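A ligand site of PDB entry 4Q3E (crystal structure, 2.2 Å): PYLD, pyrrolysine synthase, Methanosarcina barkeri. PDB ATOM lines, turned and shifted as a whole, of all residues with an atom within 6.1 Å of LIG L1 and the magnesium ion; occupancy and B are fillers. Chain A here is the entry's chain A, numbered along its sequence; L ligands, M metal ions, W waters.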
ATOM      1  N   ASN A 122      -6.611  -2.192 -11.084  1.00  0.00           N
ATOM      2  CA  ASN A 122      -7.798  -2.212 -11.936  1.00  0.00           C
ATOM      3  C   ASN A 122      -7.504  -2.142 -13.436  1.00  0.00           C
ATOM      4  O   ASN A 122      -8.171  -2.779 -14.245  1.00  0.00           O
ATOM      5  CB  ASN A 122      -8.714  -1.049 -11.528  1.00  0.00           C
ATOM      6  CG  ASN A 122      -9.883  -0.852 -12.477  1.00  0.00           C
ATOM      7  OD1 ASN A 122      -9.949   0.125 -13.212  1.00  0.00           O
ATOM      8  ND2 ASN A 122     -10.826  -1.767 -12.433  1.00  0.00           N
ATOM      9  N   GLN A 123      -6.489  -1.366 -13.807  1.00  0.00           N
ATOM     10  CA  GLN A 123      -6.200  -1.114 -15.220  1.00  0.00           C
ATOM     11  C   GLN A 123      -5.765  -2.372 -15.982  1.00  0.00           C
ATOM     12  O   GLN A 123      -6.445  -2.784 -16.938  1.00  0.00           O
ATOM     13  CB  GLN A 123      -5.217   0.055 -15.360  1.00  0.00           C
ATOM     14  CG  GLN A 123      -5.924   1.378 -15.066  1.00  0.00           C
ATOM     15  CD  GLN A 123      -5.041   2.514 -14.596  1.00  0.00           C
ATOM     16  OE1 GLN A 123      -3.870   2.335 -14.255  1.00  0.00           O
ATOM     17  NE2 GLN A 123      -5.611   3.697 -14.554  1.00  0.00           N
ATOM     18  N   THR A 126      -8.583  -5.057 -15.945  1.00  0.00           N
ATOM     19  CA  THR A 126      -9.687  -4.752 -16.851  1.00  0.00           C
ATOM     20  C   THR A 126      -9.337  -5.068 -18.298  1.00  0.00           C
ATOM     21  O   THR A 126     -10.135  -5.667 -19.009  1.00  0.00           O
ATOM     22  CB  THR A 126     -10.096  -3.279 -16.740  1.00  0.00           C
ATOM     23  OG1 THR A 126     -10.649  -3.033 -15.433  1.00  0.00           O
ATOM     24  CG2 THR A 126     -11.123  -2.936 -17.805  1.00  0.00           C
ATOM     25  N   TYR A 130     -11.251  -8.178 -20.460  1.00  0.00           N
ATOM     26  CA  TYR A 130     -12.000  -7.829 -21.666  1.00  0.00           C
ATOM     27  C   TYR A 130     -11.352  -8.439 -22.908  1.00  0.00           C
ATOM     28  O   TYR A 130     -12.051  -8.848 -23.832  1.00  0.00           O
ATOM     29  CB  TYR A 130     -12.158  -6.317 -21.813  1.00  0.00           C
ATOM     30  CG  TYR A 130     -13.334  -5.740 -21.035  1.00  0.00           C
ATOM     31  CD1 TYR A 130     -13.197  -5.345 -19.714  1.00  0.00           C
ATOM     32  CD2 TYR A 130     -14.586  -5.589 -21.638  1.00  0.00           C
ATOM     33  CE1 TYR A 130     -14.258  -4.828 -19.006  1.00  0.00           C
ATOM     34  CE2 TYR A 130     -15.656  -5.068 -20.930  1.00  0.00           C
ATOM     35  CZ  TYR A 130     -15.494  -4.693 -19.618  1.00  0.00           C
ATOM     36  OH  TYR A 130     -16.543  -4.169 -18.912  1.00  0.00           O
ATOM     37  N   VAL A 148      -7.952  -1.244 -30.172  1.00  0.00           N
ATOM     38  CA  VAL A 148      -7.967   0.221 -30.304  1.00  0.00           C
ATOM     39  C   VAL A 148      -7.811   0.848 -28.920  1.00  0.00           C
ATOM     40  O   VAL A 148      -8.681   0.717 -28.068  1.00  0.00           O
ATOM     41  CB  VAL A 148      -9.234   0.726 -31.009  1.00  0.00           C
ATOM     42  CG1 VAL A 148      -9.217   2.259 -31.127  1.00  0.00           C
ATOM     43  CG2 VAL A 148      -9.334   0.112 -32.402  1.00  0.00           C
ATOM     44  N   GLY A 149      -6.685   1.534 -28.720  1.00  0.00           N
ATOM     45  CA  GLY A 149      -6.310   2.069 -27.420  1.00  0.00           C
ATOM     46  C   GLY A 149      -5.264   1.173 -26.789  1.00  0.00           C
ATOM     47  O   GLY A 149      -5.523   0.000 -26.514  1.00  0.00           O
ATOM     48  N   LEU A 150      -4.062   1.728 -26.600  1.00  0.00           N
ATOM     49  CA  LEU A 150      -2.940   0.991 -26.019  1.00  0.00           C
ATOM     50  C   LEU A 150      -2.398   1.716 -24.795  1.00  0.00           C
ATOM     51  O   LEU A 150      -1.195   1.769 -24.567  1.00  0.00           O
ATOM     52  CB  LEU A 150      -1.841   0.795 -27.083  1.00  0.00           C
ATOM     53  CG  LEU A 150      -2.265  -0.026 -28.299  1.00  0.00           C
ATOM     54  CD1 LEU A 150      -1.321   0.156 -29.486  1.00  0.00           C
ATOM     55  CD2 LEU A 150      -2.379  -1.497 -27.938  1.00  0.00           C
ATOM     56  N   GLY A 151      -3.312   2.297 -24.002  1.00  0.00           N
ATOM     57  CA  GLY A 151      -2.952   2.924 -22.740  1.00  0.00           C
ATOM     58  C   GLY A 151      -2.878   1.918 -21.610  1.00  0.00           C
ATOM     59  O   GLY A 151      -2.540   0.752 -21.817  1.00  0.00           O
ATOM     60  N   LYS A 152      -3.217   2.378 -20.409  1.00  0.00           N
ATOM     61  CA  LYS A 152      -3.048   1.579 -19.187  1.00  0.00           C
ATOM     62  C   LYS A 152      -3.948   0.347 -19.124  1.00  0.00           C
ATOM     63  O   LYS A 152      -3.599  -0.649 -18.495  1.00  0.00           O
ATOM     64  CB  LYS A 152      -3.239   2.464 -17.943  1.00  0.00           C
ATOM     65  CG  LYS A 152      -2.200   3.583 -17.863  1.00  0.00           C
ATOM     66  CD  LYS A 152      -2.322   4.458 -16.624  1.00  0.00           C
ATOM     67  CE  LYS A 152      -3.532   5.386 -16.672  1.00  0.00           C
ATOM     68  NZ  LYS A 152      -3.466   6.403 -17.767  1.00  0.00           N
ATOM     69  N   VAL A 153      -5.093   0.409 -19.802  1.00  0.00           N
ATOM     70  CA  VAL A 153      -5.977  -0.742 -19.921  1.00  0.00           C
ATOM     71  C   VAL A 153      -5.690  -1.507 -21.219  1.00  0.00           C
ATOM     72  O   VAL A 153      -5.599  -2.727 -21.226  1.00  0.00           O
ATOM     73  CB  VAL A 153      -7.454  -0.310 -19.862  1.00  0.00           C
ATOM     74  CG1 VAL A 153      -8.406  -1.453 -20.171  1.00  0.00           C
ATOM     75  CG2 VAL A 153      -7.770   0.277 -18.494  1.00  0.00           C
ATOM     76  N   GLY A 154      -5.526  -0.762 -22.309  1.00  0.00           N
ATOM     77  CA  GLY A 154      -5.374  -1.345 -23.631  1.00  0.00           C
ATOM     78  C   GLY A 154      -4.110  -2.169 -23.805  1.00  0.00           C
ATOM     79  O   GLY A 154      -4.159  -3.255 -24.369  1.00  0.00           O
ATOM     80  N   TYR A 171      -3.909  -0.046 -32.745  1.00  0.00           N
ATOM     81  CA  TYR A 171      -3.854   1.363 -33.078  1.00  0.00           C
ATOM     82  C   TYR A 171      -4.097   2.218 -31.843  1.00  0.00           C
ATOM     83  O   TYR A 171      -4.949   1.897 -31.006  1.00  0.00           O
ATOM     84  CB  TYR A 171      -4.868   1.718 -34.167  1.00  0.00           C
ATOM     85  CG  TYR A 171      -4.886   3.194 -34.485  1.00  0.00           C
ATOM     86  CD1 TYR A 171      -3.800   3.790 -35.135  1.00  0.00           C
ATOM     87  CD2 TYR A 171      -5.952   3.993 -34.131  1.00  0.00           C
ATOM     88  CE1 TYR A 171      -3.799   5.150 -35.421  1.00  0.00           C
ATOM     89  CE2 TYR A 171      -5.964   5.347 -34.415  1.00  0.00           C
ATOM     90  CZ  TYR A 171      -4.894   5.917 -35.058  1.00  0.00           C
ATOM     91  OH  TYR A 171      -4.908   7.258 -35.308  1.00  0.00           O
ATOM     92  N   ASP A 172      -3.330   3.292 -31.738  1.00  0.00           N
ATOM     93  CA  ASP A 172      -3.573   4.318 -30.733  1.00  0.00           C
ATOM     94  C   ASP A 172      -3.262   5.650 -31.403  1.00  0.00           C
ATOM     95  O   ASP A 172      -2.294   5.748 -32.145  1.00  0.00           O
ATOM     96  CB  ASP A 172      -2.650   4.100 -29.529  1.00  0.00           C
ATOM     97  CG  ASP A 172      -3.018   4.965 -28.356  1.00  0.00           C
ATOM     98  OD1 ASP A 172      -2.857   6.206 -28.460  1.00  0.00           O
ATOM     99  OD2 ASP A 172      -3.467   4.427 -27.321  1.00  0.00           O
ATOM    100  N   ALA A 173      -4.080   6.667 -31.139  1.00  0.00           N
ATOM    101  CA  ALA A 173      -3.908   7.984 -31.772  1.00  0.00           C
ATOM    102  C   ALA A 173      -2.687   8.737 -31.257  1.00  0.00           C
ATOM    103  O   ALA A 173      -2.282   9.739 -31.860  1.00  0.00           O
ATOM    104  CB  ALA A 173      -5.165   8.829 -31.593  1.00  0.00           C
ATOM    105  N   ASP A 174      -2.129   8.283 -30.144  1.00  0.00           N
ATOM    106  CA  ASP A 174      -0.859   8.776 -29.632  1.00  0.00           C
ATOM    107  C   ASP A 174       0.260   7.990 -30.322  1.00  0.00           C
ATOM    108  O   ASP A 174       0.446   6.803 -30.027  1.00  0.00           O
ATOM    109  CB  ASP A 174      -0.822   8.585 -28.110  1.00  0.00           C
ATOM    110  CG  ASP A 174       0.439   9.102 -27.459  1.00  0.00           C
ATOM    111  OD1 ASP A 174       1.442   9.347 -28.162  1.00  0.00           O
ATOM    112  OD2 ASP A 174       0.436   9.242 -26.216  1.00  0.00           O
ATOM    113  N   LEU A 177       3.210   6.283 -28.290  1.00  0.00           N
ATOM    114  CA  LEU A 177       2.738   5.110 -27.584  1.00  0.00           C
ATOM    115  C   LEU A 177       2.544   3.934 -28.536  1.00  0.00           C
ATOM    116  O   LEU A 177       2.863   2.804 -28.194  1.00  0.00           O
ATOM    117  CB  LEU A 177       1.421   5.427 -26.861  1.00  0.00           C
ATOM    118  CG  LEU A 177       0.891   4.469 -25.804  1.00  0.00           C
ATOM    119  CD1 LEU A 177       1.947   4.124 -24.763  1.00  0.00           C
ATOM    120  CD2 LEU A 177      -0.324   5.107 -25.136  1.00  0.00           C
ATOM    121  N   ALA A 204     -10.238   0.177 -25.774  1.00  0.00           N
ATOM    122  CA  ALA A 204     -10.058   0.791 -24.461  1.00  0.00           C
ATOM    123  C   ALA A 204      -9.615   2.250 -24.565  1.00  0.00           C
ATOM    124  O   ALA A 204      -8.448   2.565 -24.304  1.00  0.00           O
ATOM    125  CB  ALA A 204      -9.050  -0.009 -23.650  1.00  0.00           C
ATOM    126  N   THR A 205     -10.539   3.136 -24.951  1.00  0.00           N
ATOM    127  CA  THR A 205     -10.275   4.571 -24.961  1.00  0.00           C
ATOM    128  C   THR A 205     -11.392   5.322 -24.233  1.00  0.00           C
ATOM    129  O   THR A 205     -12.473   4.771 -24.024  1.00  0.00           O
ATOM    130  CB  THR A 205     -10.203   5.157 -26.389  1.00  0.00           C
ATOM    131  OG1 THR A 205     -11.524   5.346 -26.911  1.00  0.00           O
ATOM    132  CG2 THR A 205      -9.400   4.248 -27.309  1.00  0.00           C
ATOM    133  N   PRO A 206     -11.140   6.595 -23.851  1.00  0.00           N
ATOM    134  CA  PRO A 206     -12.187   7.429 -23.280  1.00  0.00           C
ATOM    135  C   PRO A 206     -12.984   8.234 -24.318  1.00  0.00           C
ATOM    136  O   PRO A 206     -13.581   9.248 -23.983  1.00  0.00           O
ATOM    137  CB  PRO A 206     -11.416   8.367 -22.327  1.00  0.00           C
ATOM    138  CG  PRO A 206     -10.051   8.481 -22.927  1.00  0.00           C
ATOM    139  CD  PRO A 206      -9.809   7.249 -23.767  1.00  0.00           C
ATOM    140  N   CYS A 207     -13.016   7.761 -25.572  1.00  0.00           N
ATOM    141  CA  CYS A 207     -13.555   8.529 -26.689  1.00  0.00           C
ATOM    142  C   CYS A 207     -14.618   7.785 -27.478  1.00  0.00           C
ATOM    143  O   CYS A 207     -14.553   6.567 -27.647  1.00  0.00           O
ATOM    144  CB  CYS A 207     -12.419   8.906 -27.627  1.00  0.00           C
ATOM    145  SG  CYS A 207     -11.065   9.786 -26.813  1.00  0.00           S
ATOM    146  N   ALA A 208     -15.595   8.541 -27.986  1.00  0.00           N
ATOM    147  CA  ALA A 208     -16.628   7.981 -28.866  1.00  0.00           C
ATOM    148  C   ALA A 208     -16.120   7.847 -30.294  1.00  0.00           C
ATOM    149  O   ALA A 208     -15.149   8.508 -30.669  1.00  0.00           O
ATOM    150  CB  ALA A 208     -17.884   8.852 -28.847  1.00  0.00           C
ATOM    151  N   ASN A 209     -16.755   6.957 -31.055  1.00  0.00           N
ATOM    152  CA  ASN A 209     -16.502   6.807 -32.496  1.00  0.00           C
ATOM    153  C   ASN A 209     -15.065   6.461 -32.876  1.00  0.00           C
ATOM    154  O   ASN A 209     -14.510   7.024 -33.814  1.00  0.00           O
ATOM    155  CB  ASN A 209     -16.946   8.066 -33.261  1.00  0.00           C
ATOM    156  CG  ASN A 209     -18.405   8.398 -33.060  1.00  0.00           C
ATOM    157  OD1 ASN A 209     -19.194   7.592 -32.541  1.00  0.00           O
ATOM    158  ND2 ASN A 209     -18.792   9.592 -33.479  1.00  0.00           N
ATOM    159  N   THR A 210     -14.478   5.516 -32.147  1.00  0.00           N
ATOM    160  CA  THR A 210     -13.084   5.110 -32.378  1.00  0.00           C
ATOM    161  C   THR A 210     -12.947   3.883 -33.280  1.00  0.00           C
ATOM    162  O   THR A 210     -11.846   3.532 -33.677  1.00  0.00           O
ATOM    163  CB  THR A 210     -12.408   4.779 -31.045  1.00  0.00           C
ATOM    164  OG1 THR A 210     -13.152   3.749 -30.382  1.00  0.00           O
ATOM    165  CG2 THR A 210     -12.356   6.012 -30.163  1.00  0.00           C
ATOM    166  N   THR A 224     -15.301  -3.879 -24.928  1.00  0.00           N
ATOM    167  CA  THR A 224     -14.775  -2.553 -24.584  1.00  0.00           C
ATOM    168  C   THR A 224     -15.156  -2.088 -23.174  1.00  0.00           C
ATOM    169  O   THR A 224     -16.333  -1.988 -22.852  1.00  0.00           O
ATOM    170  CB  THR A 224     -15.204  -1.491 -25.628  1.00  0.00           C
ATOM    171  OG1 THR A 224     -14.698  -0.206 -25.253  1.00  0.00           O
ATOM    172  CG2 THR A 224     -16.730  -1.411 -25.770  1.00  0.00           C
ATOM    173  N   PRO A 225     -14.144  -1.808 -22.337  1.00  0.00           N
ATOM    174  CA  PRO A 225     -14.391  -1.117 -21.079  1.00  0.00           C
ATOM    175  C   PRO A 225     -14.456   0.396 -21.247  1.00  0.00           C
ATOM    176  O   PRO A 225     -14.774   1.101 -20.292  1.00  0.00           O
ATOM    177  CB  PRO A 225     -13.166  -1.461 -20.239  1.00  0.00           C
ATOM    178  CG  PRO A 225     -12.083  -1.616 -21.238  1.00  0.00           C
ATOM    179  CD  PRO A 225     -12.732  -2.243 -22.441  1.00  0.00           C
ATOM    180  N   GLY A 226     -14.136   0.903 -22.437  1.00  0.00           N
ATOM    181  CA  GLY A 226     -14.088   2.347 -22.674  1.00  0.00           C
ATOM    182  C   GLY A 226     -15.417   3.050 -22.459  1.00  0.00           C
ATOM    183  O   GLY A 226     -16.486   2.442 -22.578  1.00  0.00           O
ATOM    184  N   ILE A 227     -15.340   4.338 -22.134  1.00  0.00           N
ATOM    185  CA  ILE A 227     -16.503   5.171 -21.849  1.00  0.00           C
ATOM    186  C   ILE A 227     -16.258   6.554 -22.472  1.00  0.00           C
ATOM    187  O   ILE A 227     -15.210   7.145 -22.225  1.00  0.00           O
ATOM    188  CB  ILE A 227     -16.696   5.335 -20.315  1.00  0.00           C
ATOM    189  CG1 ILE A 227     -16.758   3.959 -19.619  1.00  0.00           C
ATOM    190  CG2 ILE A 227     -17.982   6.105 -20.036  1.00  0.00           C
ATOM    191  CD1 ILE A 227     -16.531   3.996 -18.122  1.00  0.00           C
ATOM    192  N   PRO A 228     -17.199   7.083 -23.275  1.00  0.00           N
ATOM    193  CA  PRO A 228     -18.474   6.531 -23.723  1.00  0.00           C
ATOM    194  C   PRO A 228     -18.263   5.432 -24.762  1.00  0.00           C
ATOM    195  O   PRO A 228     -17.126   5.036 -24.989  1.00  0.00           O
ATOM    196  CB  PRO A 228     -19.165   7.744 -24.342  1.00  0.00           C
ATOM    197  CG  PRO A 228     -18.058   8.603 -24.842  1.00  0.00           C
ATOM    198  CD  PRO A 228     -16.944   8.424 -23.840  1.00  0.00           C
ATOM    199  N   GLU A 246     -19.361  -2.733 -19.836  1.00  0.00           N
ATOM    200  CA  GLU A 246     -19.964  -2.548 -18.532  1.00  0.00           C
ATOM    201  C   GLU A 246     -19.044  -1.624 -17.694  1.00  0.00           C
ATOM    202  O   GLU A 246     -17.824  -1.717 -17.796  1.00  0.00           O
ATOM    203  CB  GLU A 246     -20.174  -3.921 -17.915  1.00  0.00           C
ATOM    204  CG  GLU A 246     -20.851  -3.926 -16.555  1.00  0.00           C
ATOM    205  CD  GLU A 246     -19.871  -3.649 -15.447  1.00  0.00           C
ATOM    206  OE1 GLU A 246     -20.250  -3.014 -14.452  1.00  0.00           O
ATOM    207  OE2 GLU A 246     -18.693  -4.059 -15.594  1.00  0.00           O
ATOM    208  N   PRO A 247     -19.636  -0.726 -16.885  1.00  0.00           N
ATOM    209  CA  PRO A 247     -18.849   0.391 -16.339  1.00  0.00           C
ATOM    210  C   PRO A 247     -17.789   0.092 -15.276  1.00  0.00           C
ATOM    211  O   PRO A 247     -16.864   0.878 -15.118  1.00  0.00           O
ATOM    212  CB  PRO A 247     -19.929   1.322 -15.754  1.00  0.00           C
ATOM    213  CG  PRO A 247     -21.238   0.844 -16.296  1.00  0.00           C
ATOM    214  CD  PRO A 247     -21.070  -0.615 -16.549  1.00  0.00           C
ATOM    215  N   LEU A 248     -17.887  -1.022 -14.548  1.00  0.00           N
ATOM    216  CA  LEU A 248     -17.051  -1.214 -13.341  1.00  0.00           C
ATOM    217  C   LEU A 248     -16.924  -2.663 -12.865  1.00  0.00           C
ATOM    218  O   LEU A 248     -15.850  -3.078 -12.426  1.00  0.00           O
ATOM    219  CB  LEU A 248     -17.625  -0.340 -12.201  1.00  0.00           C
ATOM    220  CG  LEU A 248     -16.848  -0.288 -10.884  1.00  0.00           C
ATOM    221  CD1 LEU A 248     -15.408   0.172 -11.090  1.00  0.00           C
ATOM    222  CD2 LEU A 248     -17.571   0.639  -9.924  1.00  0.00           C
ATOM    223  N   GLY A 249     -18.010  -3.409 -12.913  1.00  0.00           N
ATOM    224  CA  GLY A 249     -18.062  -4.738 -12.320  1.00  0.00           C
ATOM    225  C   GLY A 249     -17.145  -5.801 -12.892  1.00  0.00           C
ATOM    226  O   GLY A 249     -16.561  -6.581 -12.146  1.00  0.00           O
ATOM    227  N   ILE A 250     -17.050  -5.866 -14.211  1.00  0.00           N
ATOM    228  CA  ILE A 250     -16.248  -6.922 -14.845  1.00  0.00           C
ATOM    229  C   ILE A 250     -14.781  -6.775 -14.437  1.00  0.00           C
ATOM    230  O   ILE A 250     -14.133  -7.752 -14.046  1.00  0.00           O
ATOM    231  CB  ILE A 250     -16.394  -6.926 -16.378  1.00  0.00           C
ATOM    232  CG1 ILE A 250     -17.844  -7.233 -16.766  1.00  0.00           C
ATOM    233  CG2 ILE A 250     -15.456  -7.946 -17.013  1.00  0.00           C
ATOM    234  CD1 ILE A 250     -18.068  -7.406 -18.247  1.00  0.00           C
ATOM    235  N   GLY A 251     -14.279  -5.550 -14.510  1.00  0.00           N
ATOM    236  CA  GLY A 251     -12.907  -5.266 -14.089  1.00  0.00           C
ATOM    237  C   GLY A 251     -12.695  -5.562 -12.625  1.00  0.00           C
ATOM    238  O   GLY A 251     -11.655  -6.086 -12.232  1.00  0.00           O
ATOM    239  N   THR A 252     -13.684  -5.241 -11.802  1.00  0.00           N
ATOM    240  CA  THR A 252     -13.606  -5.522 -10.389  1.00  0.00           C
ATOM    241  C   THR A 252     -13.557  -7.030 -10.129  1.00  0.00           C
ATOM    242  O   THR A 252     -12.781  -7.485  -9.304  1.00  0.00           O
ATOM    243  CB  THR A 252     -14.805  -4.912  -9.635  1.00  0.00           C
ATOM    244  OG1 THR A 252     -14.854  -3.512  -9.904  1.00  0.00           O
ATOM    245  CG2 THR A 252     -14.666  -5.145  -8.125  1.00  0.00           C
HETATM  246  P1  LIG L   1      -5.439   5.879 -21.022  1.00  0.00           P
HETATM  247  O1  LIG L   1      -5.478   7.365 -21.135  1.00  0.00           O
HETATM  248  O2  LIG L   1      -4.288   5.196 -20.352  1.00  0.00           O
HETATM  249  O3  LIG L   1      -5.525   5.215 -22.478  1.00  0.00           O
HETATM  250  C1  LIG L   1      -6.472   5.670 -23.419  1.00  0.00           C
HETATM  251  C2  LIG L   1      -5.793   5.644 -24.773  1.00  0.00           C
HETATM  252  O4  LIG L   1      -6.751   5.826 -25.802  1.00  0.00           O
HETATM  253  C3  LIG L   1      -4.758   6.748 -24.947  1.00  0.00           C
HETATM  254  O5  LIG L   1      -3.468   6.153 -25.108  1.00  0.00           O
HETATM  255  C4  LIG L   1      -5.181   7.505 -26.197  1.00  0.00           C
HETATM  256  O6  LIG L   1      -4.084   7.908 -27.023  1.00  0.00           O
HETATM  257  C5  LIG L   1      -6.081   6.478 -26.862  1.00  0.00           C
HETATM  258  N1  LIG L   1      -7.058   7.048 -27.803  1.00  0.00           N
HETATM  259  C6  LIG L   1      -7.839   8.130 -27.628  1.00  0.00           C
HETATM  260  N2  LIG L   1      -8.602   8.346 -28.734  1.00  0.00           N
HETATM  261  C7  LIG L   1      -8.304   7.384 -29.624  1.00  0.00           C
HETATM  262  C8  LIG L   1      -8.729   7.009 -30.982  1.00  0.00           C
HETATM  263  N3  LIG L   1      -9.664   7.746 -31.613  1.00  0.00           N
HETATM  264  N4  LIG L   1      -8.174   5.919 -31.564  1.00  0.00           N
HETATM  265  C9  LIG L   1      -7.238   5.182 -30.933  1.00  0.00           C
HETATM  266  N5  LIG L   1      -6.801   5.473 -29.693  1.00  0.00           N
HETATM  267  C10 LIG L   1      -7.287   6.535 -29.009  1.00  0.00           C
HETATM  268  O7  LIG L   1      -6.836   5.400 -20.386  1.00  0.00           O
HETATM  269  P2  LIG L   1      -7.030   3.934 -19.730  1.00  0.00           P
HETATM  270  O8  LIG L   1      -6.555   4.045 -18.303  1.00  0.00           O
HETATM  271  O9  LIG L   1      -6.446   2.885 -20.652  1.00  0.00           O
HETATM  272  O10 LIG L   1      -8.632   3.877 -19.734  1.00  0.00           O
HETATM  273  C11 LIG L   1      -9.344   3.640 -20.938  1.00  0.00           C
HETATM  274  C12 LIG L   1     -10.842   3.837 -20.726  1.00  0.00           C
HETATM  275  O11 LIG L   1     -11.377   2.760 -19.962  1.00  0.00           O
HETATM  276  C13 LIG L   1     -11.233   5.104 -19.960  1.00  0.00           C
HETATM  277  O12 LIG L   1     -12.463   5.571 -20.507  1.00  0.00           O
HETATM  278  C14 LIG L   1     -11.472   4.628 -18.538  1.00  0.00           C
HETATM  279  O13 LIG L   1     -12.371   5.488 -17.854  1.00  0.00           O
HETATM  280  C15 LIG L   1     -12.080   3.266 -18.816  1.00  0.00           C
HETATM  281  N6  LIG L   1     -12.025   2.244 -17.783  1.00  0.00           N
HETATM  282  C16 LIG L   1     -13.115   1.461 -17.670  1.00  0.00           C
HETATM  283  C17 LIG L   1     -13.203   0.430 -16.754  1.00  0.00           C
HETATM  284  C18 LIG L   1     -14.452  -0.426 -16.692  1.00  0.00           C
HETATM  285  O14 LIG L   1     -14.573  -1.249 -15.795  1.00  0.00           O
HETATM  286  N7  LIG L   1     -15.398  -0.322 -17.634  1.00  0.00           N
HETATM  287  C19 LIG L   1     -12.041   0.143 -15.838  1.00  0.00           C
HETATM  288  C20 LIG L   1     -10.903   1.034 -16.070  1.00  0.00           C
HETATM  289  C21 LIG L   1     -10.940   2.036 -17.029  1.00  0.00           C
HETATM  290  O1  LG2 L   2     -13.550   6.291  -2.890  1.00  0.00           O
HETATM  291  C1  LG2 L   2     -13.913   7.155  -3.696  1.00  0.00           C
HETATM  292  O2  LG2 L   2     -15.155   7.607  -3.634  1.00  0.00           O
HETATM  293  C2  LG2 L   2     -12.996   7.726  -4.754  1.00  0.00           C
HETATM  294  N1  LG2 L   2     -11.657   7.956  -4.237  1.00  0.00           N
HETATM  295  C3  LG2 L   2     -12.967   6.737  -5.910  1.00  0.00           C
HETATM  296  C4  LG2 L   2     -12.159   7.173  -7.134  1.00  0.00           C
HETATM  297  C5  LG2 L   2     -12.336   6.067  -8.174  1.00  0.00           C
HETATM  298  N2  LG2 L   2     -11.526   6.147  -9.368  1.00  0.00           N
HETATM  299  C6  LG2 L   2     -11.931   6.800 -10.444  1.00  0.00           C
HETATM  300  O3  LG2 L   2     -12.955   7.471 -10.458  1.00  0.00           O
HETATM  301  C7  LG2 L   2     -11.115   6.660 -11.707  1.00  0.00           C
HETATM  302  N3  LG2 L   2     -10.767   7.985 -12.185  1.00  0.00           N
HETATM  303  C8  LG2 L   2     -11.914   5.933 -12.792  1.00  0.00           C
HETATM  304  C9  LG2 L   2     -11.923   4.417 -12.637  1.00  0.00           C
HETATM  305  C10 LG2 L   2     -12.285   3.716 -13.945  1.00  0.00           C
HETATM  306  C11 LG2 L   2     -13.783   3.809 -14.276  1.00  0.00           C
HETATM  307  N4  LG2 L   2     -13.991   4.383 -15.592  1.00  0.00           N
HETATM  308 MG    MG M   1     -15.994  -3.368 -16.249  1.00  0.00          MG
HETATM  309  O   HOH W   1     -10.674   9.966 -30.343  1.00  0.00           O
HETATM  310  O   HOH W   2      -4.769  10.346 -27.819  1.00  0.00           O
HETATM  311  O   HOH W   3      -6.275   6.849 -17.209  1.00  0.00           O
HETATM  312  O   HOH W   4      -8.151   3.837 -16.001  1.00  0.00           O
HETATM  313  O   HOH W   5      -6.016   1.983 -23.105  1.00  0.00           O
HETATM  314  O   HOH W   6     -13.292   7.828 -19.407  1.00  0.00           O
HETATM  315  O   HOH W   7      -1.702   5.922 -21.228  1.00  0.00           O
HETATM  316  O   HOH W   8     -13.519  -1.960 -13.438  1.00  0.00           O
HETATM  317  O   HOH W   9      -9.295   4.640 -33.818  1.00  0.00           O
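O14 of LIG L1 is bound to the magnesium ion, 2.6 Å away.
The magnesium ion has one donor atom within binding distance.
Slightly farther from the magnesium ion lies OH of Tyr 130 (2.8 Å).
Glu 246 touches the magnesium ion.
Leu 248 touches the magnesium ion.
Gly 249 touches the magnesium ion (N to MG, 3.9 Å).
Ile 250 touches the magnesium ion (N to MG, 3.4 Å).
Gly 251 touches the magnesium ion (N to MG, 3.3 Å).
Within 4 Å of the magnesium ion: Tyr 130, Glu 246, Leu 248, Gly 249, Ile 250 and Gly 251.
The backbone NH (N) of Asp 174 sits at hydrogen-bond distance from the side-chain carboxylate (OD1) of Asp 172, at 2.8 Å.
OE2 of Glu 246 sits at hydrogen-bond distance from N of Ile 250.
The side-chain carboxylate (OE1) of Glu 246 sits at hydrogen-bond distance from the backbone NH (N) of Gly 249, at 2.7 Å.
The backbone carbonyl oxygen (O) of Asn 122 is in hydrogen-bond range of the side-chain hydroxyl (OG1) of Thr 126, at 2.8 Å.
The side-chain hydroxyl (OG1) of Thr 205 sits at hydrogen-bond distance from the backbone NH (N) of Cys 207, at 3.1 Å.
O of Leu 248 lies within hydrogen-bond range of OG1 of Thr 252 (2.7 Å).
O of Val 148 is in hydrogen-bond range of N of Ala 204 (2.8 Å).
N of Gly 149 sits at hydrogen-bond distance from O of Tyr 171, at 2.9 Å.
Merely in contact with LIG L1: Asn 122, Leu 177, Pro 206, Thr 205, Gly 151, Leu 248, Thr 126, Asp 174, Thr 210, Ile 227, Val 148, Ala 204, Tyr 171, Gly 226 and Gln 123.
Hydrophobic or aromatic side chains within 4 Å of LIG L1: Val 148, Val 153, Tyr 171, Ala 173, Leu 177, Pro 206 and Pro 225.
23 residues have an atom within 4 Å of LIG L1: Asn 122, Gln 123, Thr 126, Val 148, Gly 151, Lys 152, Val 153, Tyr 171, Asp 172, Ala 173, Asp 174, Leu 177, Ala 204, Thr 205, Pro 206, Cys 207, Thr 210, Pro 225, Gly 226, Ile 227, Glu 246, Pro 247 and Leu 248.
The nearest printed residue that does not touch LIG L1 is Gly 149 (4.1 Å).
A nitrogen (N4) of LG2 L2 lies within hydrogen-bond range of an oxygen (O13) of LIG L1.
Water W6 lies within hydrogen-bond range of O12 of LIG L1 (2.6 Å) and O of Ile 227 (3.5 Å).
Water W5 lies within hydrogen-bond range of O9 of LIG L1 (2.6 Å), O of Ala 204 (2.8 Å), N of Gly 151 (2.9 Å) and N of Gly 154 (2.9 Å).
Water W8 bridges O of Leu 248 (2.8 Å) and ND2 of Asn 122 (2.9 Å).
Water W1 bridges N3 of LIG L1 (2.7 Å) and SG of Cys 207 (3.6 Å).
Water W4 bridges O8 of LIG L1 (2.8 Å) and NE2 of Gln 123 (2.9 Å).
Water W9 bridges the backbone carbonyl oxygen (O) of Thr 210 (2.8 Å) and a nitrogen (N4) of LIG L1 (2.8 Å).
An oxygen (O6) of LIG L1 is in hydrogen-bond range of the side-chain carboxylate (OD1) of Asp 172 (2.5 Å).
O of Glu 246 lies within hydrogen-bond range of N7 of LIG L1, at 2.8 Å.
The backbone NH (N) of Val 153 is in hydrogen-bond range of an oxygen (O9) of LIG L1.
The backbone NH (N) of Lys 152 lies within hydrogen-bond range of an oxygen (O2) of LIG L1 (3.0 Å).
An oxygen (O2) of LIG L1 lies within salt-bridge range of the side-chain amino group of Lys 152, at 3.0 Å.
The backbone carbonyl oxygen of Pro 225 lies within hydrogen-bond range of a nitrogen (N7) of LIG L1.
The backbone carbonyl oxygen of Pro 247 lies within hydrogen-bond range of a nitrogen (N7) of LIG L1, at 3.1 Å.
The backbone NH (N) of Ala 173 lies within hydrogen-bond range of a nitrogen (N5) of LIG L1, 3.3 Å away.
SG of Cys 207 is in hydrogen-bond range of N2 of LIG L1 (3.4 Å).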
